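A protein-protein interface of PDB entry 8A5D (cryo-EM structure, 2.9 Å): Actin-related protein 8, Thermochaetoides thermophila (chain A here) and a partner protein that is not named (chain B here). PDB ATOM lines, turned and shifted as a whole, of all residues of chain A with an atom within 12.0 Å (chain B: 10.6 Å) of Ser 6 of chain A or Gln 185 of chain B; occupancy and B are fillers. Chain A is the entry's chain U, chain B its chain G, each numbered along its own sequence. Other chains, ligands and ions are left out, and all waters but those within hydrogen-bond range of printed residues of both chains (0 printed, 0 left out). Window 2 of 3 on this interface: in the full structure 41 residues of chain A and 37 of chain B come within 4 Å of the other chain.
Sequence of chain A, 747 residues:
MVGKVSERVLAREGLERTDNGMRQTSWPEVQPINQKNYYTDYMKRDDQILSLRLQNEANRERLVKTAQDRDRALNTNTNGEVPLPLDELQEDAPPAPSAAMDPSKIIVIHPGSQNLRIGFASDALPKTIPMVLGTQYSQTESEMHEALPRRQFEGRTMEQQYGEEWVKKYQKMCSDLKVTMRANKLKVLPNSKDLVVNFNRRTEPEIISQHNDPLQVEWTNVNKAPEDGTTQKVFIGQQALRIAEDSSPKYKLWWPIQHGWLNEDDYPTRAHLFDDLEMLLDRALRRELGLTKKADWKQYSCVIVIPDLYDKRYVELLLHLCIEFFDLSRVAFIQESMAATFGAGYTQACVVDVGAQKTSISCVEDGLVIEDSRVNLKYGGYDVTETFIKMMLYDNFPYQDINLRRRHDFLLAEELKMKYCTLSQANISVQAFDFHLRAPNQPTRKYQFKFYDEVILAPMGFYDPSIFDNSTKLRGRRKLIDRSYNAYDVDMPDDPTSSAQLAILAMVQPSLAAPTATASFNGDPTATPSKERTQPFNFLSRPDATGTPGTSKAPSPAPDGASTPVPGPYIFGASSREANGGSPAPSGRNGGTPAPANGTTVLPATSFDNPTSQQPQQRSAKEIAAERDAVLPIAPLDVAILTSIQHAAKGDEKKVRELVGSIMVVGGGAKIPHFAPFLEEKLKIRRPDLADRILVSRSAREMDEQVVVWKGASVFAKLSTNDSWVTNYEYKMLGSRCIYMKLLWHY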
ATOM      1  N   SER A   6     -15.917 -17.668 -33.209  1.00  0.00           N
ATOM      2  CA  SER A   6     -15.962 -17.319 -31.745  1.00  0.00           C
ATOM      3  C   SER A   6     -17.374 -16.878 -31.327  1.00  0.00           C
ATOM      4  O   SER A   6     -17.966 -17.560 -30.471  1.00  0.00           O
ATOM      5  CB  SER A   6     -14.938 -16.261 -31.402  1.00  0.00           C
ATOM      6  OG  SER A   6     -14.929 -15.990 -30.005  1.00  0.00           O
ATOM      7  N   GLU A   7     -17.896 -15.792 -31.915  1.00  0.00           N
ATOM      8  CA  GLU A   7     -19.088 -15.026 -31.435  1.00  0.00           C
ATOM      9  C   GLU A   7     -20.265 -15.948 -31.067  1.00  0.00           C
ATOM     10  O   GLU A   7     -20.834 -15.757 -29.972  1.00  0.00           O
ATOM     11  CB  GLU A   7     -19.503 -13.983 -32.479  1.00  0.00           C
ATOM     12  CG  GLU A   7     -20.620 -13.048 -32.027  1.00  0.00           C
ATOM     13  CD  GLU A   7     -20.338 -12.176 -30.809  1.00  0.00           C
ATOM     14  OE1 GLU A   7     -21.315 -11.715 -30.179  1.00  0.00           O
ATOM     15  OE2 GLU A   7     -19.151 -11.945 -30.493  1.00  0.00           O
ATOM     16  N   ARG A   8     -20.631 -16.908 -31.921  1.00  0.00           N
ATOM     17  CA  ARG A   8     -21.835 -17.761 -31.703  1.00  0.00           C
ATOM     18  C   ARG A   8     -21.658 -18.682 -30.481  1.00  0.00           C
ATOM     19  O   ARG A   8     -22.691 -19.014 -29.865  1.00  0.00           O
ATOM     20  CB  ARG A   8     -22.182 -18.533 -32.981  1.00  0.00           C
ATOM     21  CG  ARG A   8     -22.720 -17.649 -34.097  1.00  0.00           C
ATOM     22  CD  ARG A   8     -23.289 -18.438 -35.266  1.00  0.00           C
ATOM     23  NE  ARG A   8     -24.073 -17.613 -36.189  1.00  0.00           N
ATOM     24  CZ  ARG A   8     -23.638 -17.049 -37.325  1.00  0.00           C
ATOM     25  NH1 ARG A   8     -22.389 -17.193 -37.745  1.00  0.00           N
ATOM     26  NH2 ARG A   8     -24.479 -16.328 -38.051  1.00  0.00           N
ATOM     27  N   VAL A   9     -20.428 -19.052 -30.098  1.00  0.00           N
ATOM     28  CA  VAL A   9     -20.164 -19.860 -28.867  1.00  0.00           C
ATOM     29  C   VAL A   9     -20.429 -18.979 -27.636  1.00  0.00           C
ATOM     30  O   VAL A   9     -21.007 -19.492 -26.652  1.00  0.00           O
ATOM     31  CB  VAL A   9     -18.744 -20.465 -28.872  1.00  0.00           C
ATOM     32  CG1 VAL A   9     -18.394 -21.142 -27.551  1.00  0.00           C
ATOM     33  CG2 VAL A   9     -18.568 -21.436 -30.030  1.00  0.00           C
ATOM     34  N   LEU A  10     -20.060 -17.695 -27.699  1.00  0.00           N
ATOM     35  CA  LEU A  10     -20.337 -16.707 -26.621  1.00  0.00           C
ATOM     36  C   LEU A  10     -21.858 -16.546 -26.490  1.00  0.00           C
ATOM     37  O   LEU A  10     -22.366 -16.671 -25.360  1.00  0.00           O
ATOM     38  CB  LEU A  10     -19.651 -15.371 -26.931  1.00  0.00           C
ATOM     39  CG  LEU A  10     -18.146 -15.425 -27.205  1.00  0.00           C
ATOM     40  CD1 LEU A  10     -17.595 -14.031 -27.473  1.00  0.00           C
ATOM     41  CD2 LEU A  10     -17.398 -16.097 -26.061  1.00  0.00           C
ATOM     42  N   ALA A  11     -22.564 -16.352 -27.609  1.00  0.00           N
ATOM     43  CA  ALA A  11     -24.043 -16.230 -27.667  1.00  0.00           C
ATOM     44  C   ALA A  11     -24.708 -17.522 -27.156  1.00  0.00           C
ATOM     45  O   ALA A  11     -25.729 -17.402 -26.444  1.00  0.00           O
ATOM     46  CB  ALA A  11     -24.485 -15.880 -29.070  1.00  0.00           C
ATOM     47  N   ARG A  12     -24.132 -18.700 -27.438  1.00  0.00           N
ATOM     48  CA  ARG A  12     -24.645 -20.020 -26.964  1.00  0.00           C
ATOM     49  C   ARG A  12     -24.490 -20.132 -25.436  1.00  0.00           C
ATOM     50  O   ARG A  12     -25.412 -20.676 -24.791  1.00  0.00           O
ATOM     51  CB  ARG A  12     -23.935 -21.161 -27.703  1.00  0.00           C
ATOM     52  CG  ARG A  12     -24.514 -22.541 -27.432  1.00  0.00           C
ATOM     53  CD  ARG A  12     -23.989 -23.580 -28.408  1.00  0.00           C
ATOM     54  NE  ARG A  12     -24.713 -24.844 -28.329  1.00  0.00           N
ATOM     55  CZ  ARG A  12     -24.479 -25.916 -29.088  1.00  0.00           C
ATOM     56  NH1 ARG A  12     -23.525 -25.902 -30.008  1.00  0.00           N
ATOM     57  NH2 ARG A  12     -25.207 -27.010 -28.923  1.00  0.00           N
ATOM     58  N   GLU A  13     -23.389 -19.620 -24.874  1.00  0.00           N
ATOM     59  CA  GLU A  13     -23.173 -19.497 -23.401  1.00  0.00           C
ATOM     60  C   GLU A  13     -24.070 -18.385 -22.816  1.00  0.00           C
ATOM     61  O   GLU A  13     -24.192 -18.313 -21.575  1.00  0.00           O
ATOM     62  CB  GLU A  13     -21.680 -19.265 -23.125  1.00  0.00           C
ATOM     63  CG  GLU A  13     -21.275 -19.331 -21.656  1.00  0.00           C
ATOM     64  CD  GLU A  13     -21.635 -20.615 -20.922  1.00  0.00           C
ATOM     65  OE1 GLU A  13     -21.776 -21.661 -21.591  1.00  0.00           O
ATOM     66  OE2 GLU A  13     -21.768 -20.570 -19.679  1.00  0.00           O
ATOM     67  N   GLY A  14     -24.677 -17.538 -23.658  1.00  0.00           N
ATOM     68  CA  GLY A  14     -25.605 -16.466 -23.249  1.00  0.00           C
ATOM     69  C   GLY A  14     -24.886 -15.164 -22.946  1.00  0.00           C
ATOM     70  O   GLY A  14     -25.550 -14.263 -22.388  1.00  0.00           O
ATOM     71  N   LEU A  15     -23.610 -15.029 -23.330  1.00  0.00           N
ATOM     72  CA  LEU A  15     -22.783 -13.829 -23.018  1.00  0.00           C
ATOM     73  C   LEU A  15     -22.731 -12.894 -24.240  1.00  0.00           C
ATOM     74  O   LEU A  15     -22.357 -13.337 -25.333  1.00  0.00           O
ATOM     75  CB  LEU A  15     -21.379 -14.244 -22.578  1.00  0.00           C
ATOM     76  CG  LEU A  15     -21.280 -15.348 -21.527  1.00  0.00           C
ATOM     77  CD1 LEU A  15     -19.825 -15.718 -21.273  1.00  0.00           C
ATOM     78  CD2 LEU A  15     -21.947 -14.958 -20.223  1.00  0.00           C
ATOM     79  N   GLU A  16     -23.100 -11.629 -24.053  1.00  0.00           N
ATOM     80  CA  GLU A  16     -23.262 -10.649 -25.155  1.00  0.00           C
ATOM     81  C   GLU A  16     -23.174  -9.217 -24.613  1.00  0.00           C
ATOM     82  O   GLU A  16     -23.942  -8.861 -23.710  1.00  0.00           O
ATOM     83  CB  GLU A  16     -24.593 -10.905 -25.856  1.00  0.00           C
ATOM     84  CG  GLU A  16     -24.991  -9.809 -26.839  1.00  0.00           C
ATOM     85  CD  GLU A  16     -26.080 -10.213 -27.821  1.00  0.00           C
ATOM     86  OE1 GLU A  16     -26.990 -10.974 -27.420  1.00  0.00           O
ATOM     87  OE2 GLU A  16     -26.009  -9.773 -28.988  1.00  0.00           O
ATOM     88  N   ARG A  17     -22.281  -8.407 -25.173  1.00  0.00           N
ATOM     89  CA  ARG A  17     -22.110  -6.997 -24.743  1.00  0.00           C
ATOM     90  C   ARG A  17     -23.156  -6.130 -25.454  1.00  0.00           C
ATOM     91  O   ARG A  17     -23.507  -6.417 -26.619  1.00  0.00           O
ATOM     92  CB  ARG A  17     -20.660  -6.526 -24.890  1.00  0.00           C
ATOM     93  CG  ARG A  17     -20.146  -6.310 -26.305  1.00  0.00           C
ATOM     94  CD  ARG A  17     -18.739  -5.739 -26.232  1.00  0.00           C
ATOM     95  NE  ARG A  17     -18.317  -5.051 -27.454  1.00  0.00           N
ATOM     96  CZ  ARG A  17     -17.511  -3.982 -27.521  1.00  0.00           C
ATOM     97  NH1 ARG A  17     -17.011  -3.426 -26.424  1.00  0.00           N
ATOM     98  NH2 ARG A  17     -17.215  -3.461 -28.702  1.00  0.00           N
ATOM     99  N   THR A  18     -23.640  -5.111 -24.740  1.00  0.00           N
ATOM    100  CA  THR A  18     -24.943  -4.441 -24.983  1.00  0.00           C
ATOM    101  C   THR A  18     -24.891  -2.961 -24.584  1.00  0.00           C
ATOM    102  O   THR A  18     -24.226  -2.580 -23.591  1.00  0.00           O
ATOM    103  CB  THR A  18     -26.075  -5.200 -24.274  1.00  0.00           C
ATOM    104  OG1 THR A  18     -27.291  -4.536 -24.623  1.00  0.00           O
ATOM    105  CG2 THR A  18     -25.932  -5.289 -22.766  1.00  0.00           C
ATOM    106  N   PHE B 178     -18.806 -19.008 -16.482  1.00  0.00           N
ATOM    107  CA  PHE B 178     -17.938 -18.010 -15.766  1.00  0.00           C
ATOM    108  C   PHE B 178     -16.448 -18.360 -15.917  1.00  0.00           C
ATOM    109  O   PHE B 178     -15.708 -17.539 -16.496  1.00  0.00           O
ATOM    110  CB  PHE B 178     -18.362 -17.883 -14.302  1.00  0.00           C
ATOM    111  CG  PHE B 178     -19.645 -17.112 -14.117  1.00  0.00           C
ATOM    112  CD1 PHE B 178     -19.632 -15.728 -14.030  1.00  0.00           C
ATOM    113  CD2 PHE B 178     -20.866 -17.769 -14.064  1.00  0.00           C
ATOM    114  CE1 PHE B 178     -20.815 -15.021 -13.864  1.00  0.00           C
ATOM    115  CE2 PHE B 178     -22.047 -17.059 -13.904  1.00  0.00           C
ATOM    116  CZ  PHE B 178     -22.019 -15.686 -13.805  1.00  0.00           C
ATOM    117  N   GLN B 179     -16.017 -19.535 -15.448  1.00  0.00           N
ATOM    118  CA  GLN B 179     -14.600 -19.991 -15.531  1.00  0.00           C
ATOM    119  C   GLN B 179     -14.326 -20.503 -16.957  1.00  0.00           C
ATOM    120  O   GLN B 179     -14.215 -21.741 -17.132  1.00  0.00           O
ATOM    121  CB  GLN B 179     -14.329 -21.046 -14.450  1.00  0.00           C
ATOM    122  CG  GLN B 179     -14.604 -20.570 -13.021  1.00  0.00           C
ATOM    123  CD  GLN B 179     -16.052 -20.654 -12.587  1.00  0.00           C
ATOM    124  OE1 GLN B 179     -16.910 -21.184 -13.290  1.00  0.00           O
ATOM    125  NE2 GLN B 179     -16.342 -20.107 -11.417  1.00  0.00           N
ATOM    126  N   SER B 180     -14.215 -19.600 -17.943  1.00  0.00           N
ATOM    127  CA  SER B 180     -13.922 -19.947 -19.364  1.00  0.00           C
ATOM    128  C   SER B 180     -13.288 -18.778 -20.134  1.00  0.00           C
ATOM    129  O   SER B 180     -13.554 -17.597 -19.802  1.00  0.00           O
ATOM    130  CB  SER B 180     -15.153 -20.461 -20.077  1.00  0.00           C
ATOM    131  OG  SER B 180     -16.045 -19.406 -20.409  1.00  0.00           O
ATOM    132  N   LYS B 181     -12.517 -19.110 -21.175  1.00  0.00           N
ATOM    133  CA  LYS B 181     -11.793 -18.137 -22.042  1.00  0.00           C
ATOM    134  C   LYS B 181     -12.790 -17.167 -22.694  1.00  0.00           C
ATOM    135  O   LYS B 181     -12.433 -15.982 -22.827  1.00  0.00           O
ATOM    136  CB  LYS B 181     -10.955 -18.866 -23.099  1.00  0.00           C
ATOM    137  CG  LYS B 181      -9.766 -19.644 -22.553  1.00  0.00           C
ATOM    138  CD  LYS B 181      -9.110 -20.560 -23.569  1.00  0.00           C
ATOM    139  CE  LYS B 181      -8.122 -21.527 -22.947  1.00  0.00           C
ATOM    140  NZ  LYS B 181      -7.568 -22.471 -23.946  1.00  0.00           N
ATOM    141  N   GLY B 182     -13.987 -17.647 -23.065  1.00  0.00           N
ATOM    142  CA  GLY B 182     -15.068 -16.837 -23.669  1.00  0.00           C
ATOM    143  C   GLY B 182     -15.528 -15.721 -22.746  1.00  0.00           C
ATOM    144  O   GLY B 182     -15.521 -14.544 -23.170  1.00  0.00           O
ATOM    145  N   TYR B 183     -15.890 -16.062 -21.512  1.00  0.00           N
ATOM    146  CA  TYR B 183     -16.333 -15.086 -20.487  1.00  0.00           C
ATOM    147  C   TYR B 183     -15.217 -14.086 -20.195  1.00  0.00           C
ATOM    148  O   TYR B 183     -15.492 -12.866 -20.228  1.00  0.00           O
ATOM    149  CB  TYR B 183     -16.731 -15.794 -19.202  1.00  0.00           C
ATOM    150  CG  TYR B 183     -17.030 -14.870 -18.052  1.00  0.00           C
ATOM    151  CD1 TYR B 183     -16.037 -14.478 -17.177  1.00  0.00           C
ATOM    152  CD2 TYR B 183     -18.316 -14.424 -17.809  1.00  0.00           C
ATOM    153  CE1 TYR B 183     -16.303 -13.648 -16.102  1.00  0.00           C
ATOM    154  CE2 TYR B 183     -18.608 -13.617 -16.723  1.00  0.00           C
ATOM    155  CZ  TYR B 183     -17.597 -13.217 -15.871  1.00  0.00           C
ATOM    156  OH  TYR B 183     -17.883 -12.395 -14.820  1.00  0.00           O
ATOM    157  N   ASN B 184     -14.000 -14.579 -19.962  1.00  0.00           N
ATOM    158  CA  ASN B 184     -12.823 -13.723 -19.678  1.00  0.00           C
ATOM    159  C   ASN B 184     -12.586 -12.753 -20.844  1.00  0.00           C
ATOM    160  O   ASN B 184     -12.318 -11.575 -20.572  1.00  0.00           O
ATOM    161  CB  ASN B 184     -11.590 -14.566 -19.362  1.00  0.00           C
ATOM    162  CG  ASN B 184     -11.685 -15.285 -18.030  1.00  0.00           C
ATOM    163  OD1 ASN B 184     -12.450 -14.893 -17.152  1.00  0.00           O
ATOM    164  ND2 ASN B 184     -10.902 -16.338 -17.860  1.00  0.00           N
ATOM    165  N   GLN B 185     -12.693 -13.209 -22.086  1.00  0.00           N
ATOM    166  CA  GLN B 185     -12.447 -12.360 -23.276  1.00  0.00           C
ATOM    167  C   GLN B 185     -13.488 -11.239 -23.315  1.00  0.00           C
ATOM    168  O   GLN B 185     -13.083 -10.085 -23.553  1.00  0.00           O
ATOM    169  CB  GLN B 185     -12.478 -13.199 -24.553  1.00  0.00           C
ATOM    170  CG  GLN B 185     -12.117 -12.420 -25.811  1.00  0.00           C
ATOM    171  CD  GLN B 185     -12.189 -13.264 -27.064  1.00  0.00           C
ATOM    172  OE1 GLN B 185     -13.049 -14.135 -27.203  1.00  0.00           O
ATOM    173  NE2 GLN B 185     -11.290 -12.999 -28.002  1.00  0.00           N
ATOM    174  N   ILE B 186     -14.771 -11.554 -23.104  1.00  0.00           N
ATOM    175  CA  ILE B 186     -15.872 -10.546 -23.167  1.00  0.00           C
ATOM    176  C   ILE B 186     -15.624  -9.493 -22.082  1.00  0.00           C
ATOM    177  O   ILE B 186     -15.624  -8.298 -22.422  1.00  0.00           O
ATOM    178  CB  ILE B 186     -17.258 -11.198 -23.043  1.00  0.00           C
ATOM    179  CG1 ILE B 186     -17.537 -12.121 -24.224  1.00  0.00           C
ATOM    180  CG2 ILE B 186     -18.348 -10.149 -22.953  1.00  0.00           C
ATOM    181  CD1 ILE B 186     -18.712 -13.033 -24.015  1.00  0.00           C
ATOM    182  N   TYR B 187     -15.452  -9.922 -20.838  1.00  0.00           N
ATOM    183  CA  TYR B 187     -15.252  -9.022 -19.682  1.00  0.00           C
ATOM    184  C   TYR B 187     -14.074  -8.093 -19.981  1.00  0.00           C
ATOM    185  O   TYR B 187     -14.248  -6.851 -19.857  1.00  0.00           O
ATOM    186  CB  TYR B 187     -15.050  -9.798 -18.380  1.00  0.00           C
ATOM    187  CG  TYR B 187     -14.855  -8.916 -17.173  1.00  0.00           C
ATOM    188  CD1 TYR B 187     -13.634  -8.307 -16.914  1.00  0.00           C
ATOM    189  CD2 TYR B 187     -15.886  -8.665 -16.290  1.00  0.00           C
ATOM    190  CE1 TYR B 187     -13.436  -7.467 -15.830  1.00  0.00           C
ATOM    191  CE2 TYR B 187     -15.708  -7.823 -15.199  1.00  0.00           C
ATOM    192  CZ  TYR B 187     -14.480  -7.220 -14.962  1.00  0.00           C
ATOM    193  OH  TYR B 187     -14.262  -6.412 -13.878  1.00  0.00           O
ATOM    194  N   ASP B 188     -12.927  -8.630 -20.379  1.00  0.00           N
ATOM    195  CA  ASP B 188     -11.720  -7.815 -20.665  1.00  0.00           C
ATOM    196  C   ASP B 188     -12.006  -6.851 -21.831  1.00  0.00           C
ATOM    197  O   ASP B 188     -11.533  -5.695 -21.775  1.00  0.00           O
ATOM    198  CB  ASP B 188     -10.507  -8.698 -20.968  1.00  0.00           C
ATOM    199  CG  ASP B 188      -9.966  -9.535 -19.805  1.00  0.00           C
ATOM    200  OD1 ASP B 188     -10.522  -9.461 -18.687  1.00  0.00           O
ATOM    201  OD2 ASP B 188      -8.975 -10.271 -20.030  1.00  0.00           O
ATOM    202  N   GLN B 189     -12.725  -7.290 -22.865  1.00  0.00           N
ATOM    203  CA  GLN B 189     -12.954  -6.488 -24.098  1.00  0.00           C
ATOM    204  C   GLN B 189     -13.890  -5.317 -23.776  1.00  0.00           C
ATOM    205  O   GLN B 189     -13.677  -4.226 -24.319  1.00  0.00           O
ATOM    206  CB  GLN B 189     -13.500  -7.409 -25.190  1.00  0.00           C
ATOM    207  CG  GLN B 189     -13.788  -6.711 -26.517  1.00  0.00           C
ATOM    208  CD  GLN B 189     -14.386  -7.638 -27.556  1.00  0.00           C
ATOM    209  OE1 GLN B 189     -14.208  -8.857 -27.514  1.00  0.00           O
ATOM    210  NE2 GLN B 189     -15.112  -7.065 -28.506  1.00  0.00           N
ATOM    211  N   ILE B 190     -14.894  -5.535 -22.928  1.00  0.00           N
ATOM    212  CA  ILE B 190     -15.794  -4.459 -22.412  1.00  0.00           C
ATOM    213  C   ILE B 190     -14.973  -3.434 -21.615  1.00  0.00           C
ATOM    214  O   ILE B 190     -15.029  -2.245 -21.951  1.00  0.00           O
ATOM    215  CB  ILE B 190     -16.957  -5.062 -21.622  1.00  0.00           C
ATOM    216  CG1 ILE B 190     -17.929  -5.716 -22.613  1.00  0.00           C
ATOM    217  CG2 ILE B 190     -17.646  -4.020 -20.776  1.00  0.00           C
ATOM    218  CD1 ILE B 190     -19.043  -6.549 -21.975  1.00  0.00           C
ATOM    219  N   TRP B 191     -14.173  -3.866 -20.667  1.00  0.00           N
ATOM    220  CA  TRP B 191     -13.372  -2.926 -19.856  1.00  0.00           C
ATOM    221  C   TRP B 191     -12.336  -2.191 -20.714  1.00  0.00           C
ATOM    222  O   TRP B 191     -12.087  -1.012 -20.426  1.00  0.00           O
ATOM    223  CB  TRP B 191     -12.765  -3.618 -18.625  1.00  0.00           C
ATOM    224  CG  TRP B 191     -13.795  -3.639 -17.563  1.00  0.00           C
ATOM    225  CD1 TRP B 191     -14.824  -4.529 -17.438  1.00  0.00           C
ATOM    226  CD2 TRP B 191     -14.037  -2.599 -16.603  1.00  0.00           C
ATOM    227  NE1 TRP B 191     -15.643  -4.162 -16.406  1.00  0.00           N
ATOM    228  CE2 TRP B 191     -15.202  -2.971 -15.893  1.00  0.00           C
ATOM    229  CE3 TRP B 191     -13.342  -1.450 -16.219  1.00  0.00           C
ATOM    230  CZ2 TRP B 191     -15.696  -2.223 -14.834  1.00  0.00           C
ATOM    231  CZ3 TRP B 191     -13.832  -0.712 -15.165  1.00  0.00           C
ATOM    232  CH2 TRP B 191     -14.999  -1.086 -14.498  1.00  0.00           C
ATOM    233  N   ARG B 192     -11.721  -2.836 -21.685  1.00  0.00           N
ATOM    234  CA  ARG B 192     -10.734  -2.164 -22.547  1.00  0.00           C
ATOM    235  C   ARG B 192     -11.427  -1.009 -23.286  1.00  0.00           C
ATOM    236  O   ARG B 192     -10.855   0.103 -23.317  1.00  0.00           O
ATOM    237  CB  ARG B 192     -10.105  -3.170 -23.500  1.00  0.00           C
ATOM    238  CG  ARG B 192      -9.235  -2.570 -24.602  1.00  0.00           C
ATOM    239  CD  ARG B 192      -8.544  -3.648 -25.424  1.00  0.00           C
ATOM    240  NE  ARG B 192      -7.714  -4.466 -24.541  1.00  0.00           N
ATOM    241  CZ  ARG B 192      -7.880  -5.775 -24.275  1.00  0.00           C
ATOM    242  NH1 ARG B 192      -8.828  -6.498 -24.868  1.00  0.00           N
ATOM    243  NH2 ARG B 192      -7.076  -6.354 -23.393  1.00  0.00           N
ATOM    244  N   ASP B 193     -12.588  -1.242 -23.888  1.00  0.00           N
ATOM    245  CA  ASP B 193     -13.298  -0.195 -24.665  1.00  0.00           C
ATOM    246  C   ASP B 193     -13.794   0.896 -23.712  1.00  0.00           C
ATOM    247  O   ASP B 193     -13.661   2.072 -24.057  1.00  0.00           O
ATOM    248  CB  ASP B 193     -14.394  -0.826 -25.521  1.00  0.00           C
ATOM    249  CG  ASP B 193     -13.856  -1.570 -26.743  1.00  0.00           C
ATOM    250  OD1 ASP B 193     -12.635  -1.462 -27.024  1.00  0.00           O
ATOM    251  OD2 ASP B 193     -14.666  -2.236 -27.430  1.00  0.00           O
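The backbone NH of Leu 15 of chain A sits at hydrogen-bond distance from the backbone carbonyl oxygen of Leu 10 of chain A (2.9 Å).
Among the printed residues, pairs that only touch across the chains: Leu 15 of chain A with Ile 186 of chain B, Arg 17 of chain A with Ile 190 of chain B, Leu 10 of chain A with Gly 182 of chain B, Leu 15 of chain A with Tyr 183 of chain B, Leu 10 of chain A with Ile 186 of chain B, Ser 6 of chain A with Gln 185 of chain B and Arg 17 of chain A with Gln 189 of chain B.
The guanidinium group of Arg 17 of chain A lies within salt-bridge range of the side-chain carboxylate of Asp 193 of chain B, 2.8 Å away.
Hydrophobic or aromatic side chains of chain B that line the printed part of chain A: Tyr 183, Ile 186 and Ile 190.
Hydrophobic or aromatic side chains of chain A within 4 Å of the printed part of chain B: Leu 10 and Leu 15.
Among the printed residues, 8 pairs touch across the chains.
Among the printed residues, Asp or Glu carboxylates within 4 Å of a Lys or Arg side-chain nitrogen of the other chain: Arg 17 of chain A with Asp 193 of chain B (2.8 Å).
Ser 6 of chain A touches just one residue of chain B: Gln 185 (3.9 Å).
Gln 185 of chain B touches one residue of chain A.
No residue of chain B comes within 4 Å of Val 9 of chain A.
No residue of chain A comes within 4 Å of Asn 184 of chain B.
Of chain A, only Leu 10 and Leu 15 come within 4 Å of Ile 186 of chain B.
Of the printed residues of chain A, Asp 193 of chain B touches Arg 17.
Of the printed residues of chain B, Leu 10 of chain A touches Gly 182 and Ile 186.
Of the printed residues of chain A, Ile 190 of chain B touches Arg 17.
Of the printed residues of chain B, Leu 15 of chain A touches Tyr 183 and Ile 186.
The nearest residue of chain A that does not touch Gln 185 of chain B is Leu 10 of chain A (4.6 Å).
The nearest printed residue of chain B that does not touch Leu 10 of chain A is Gln 185 of chain B (4.6 Å).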
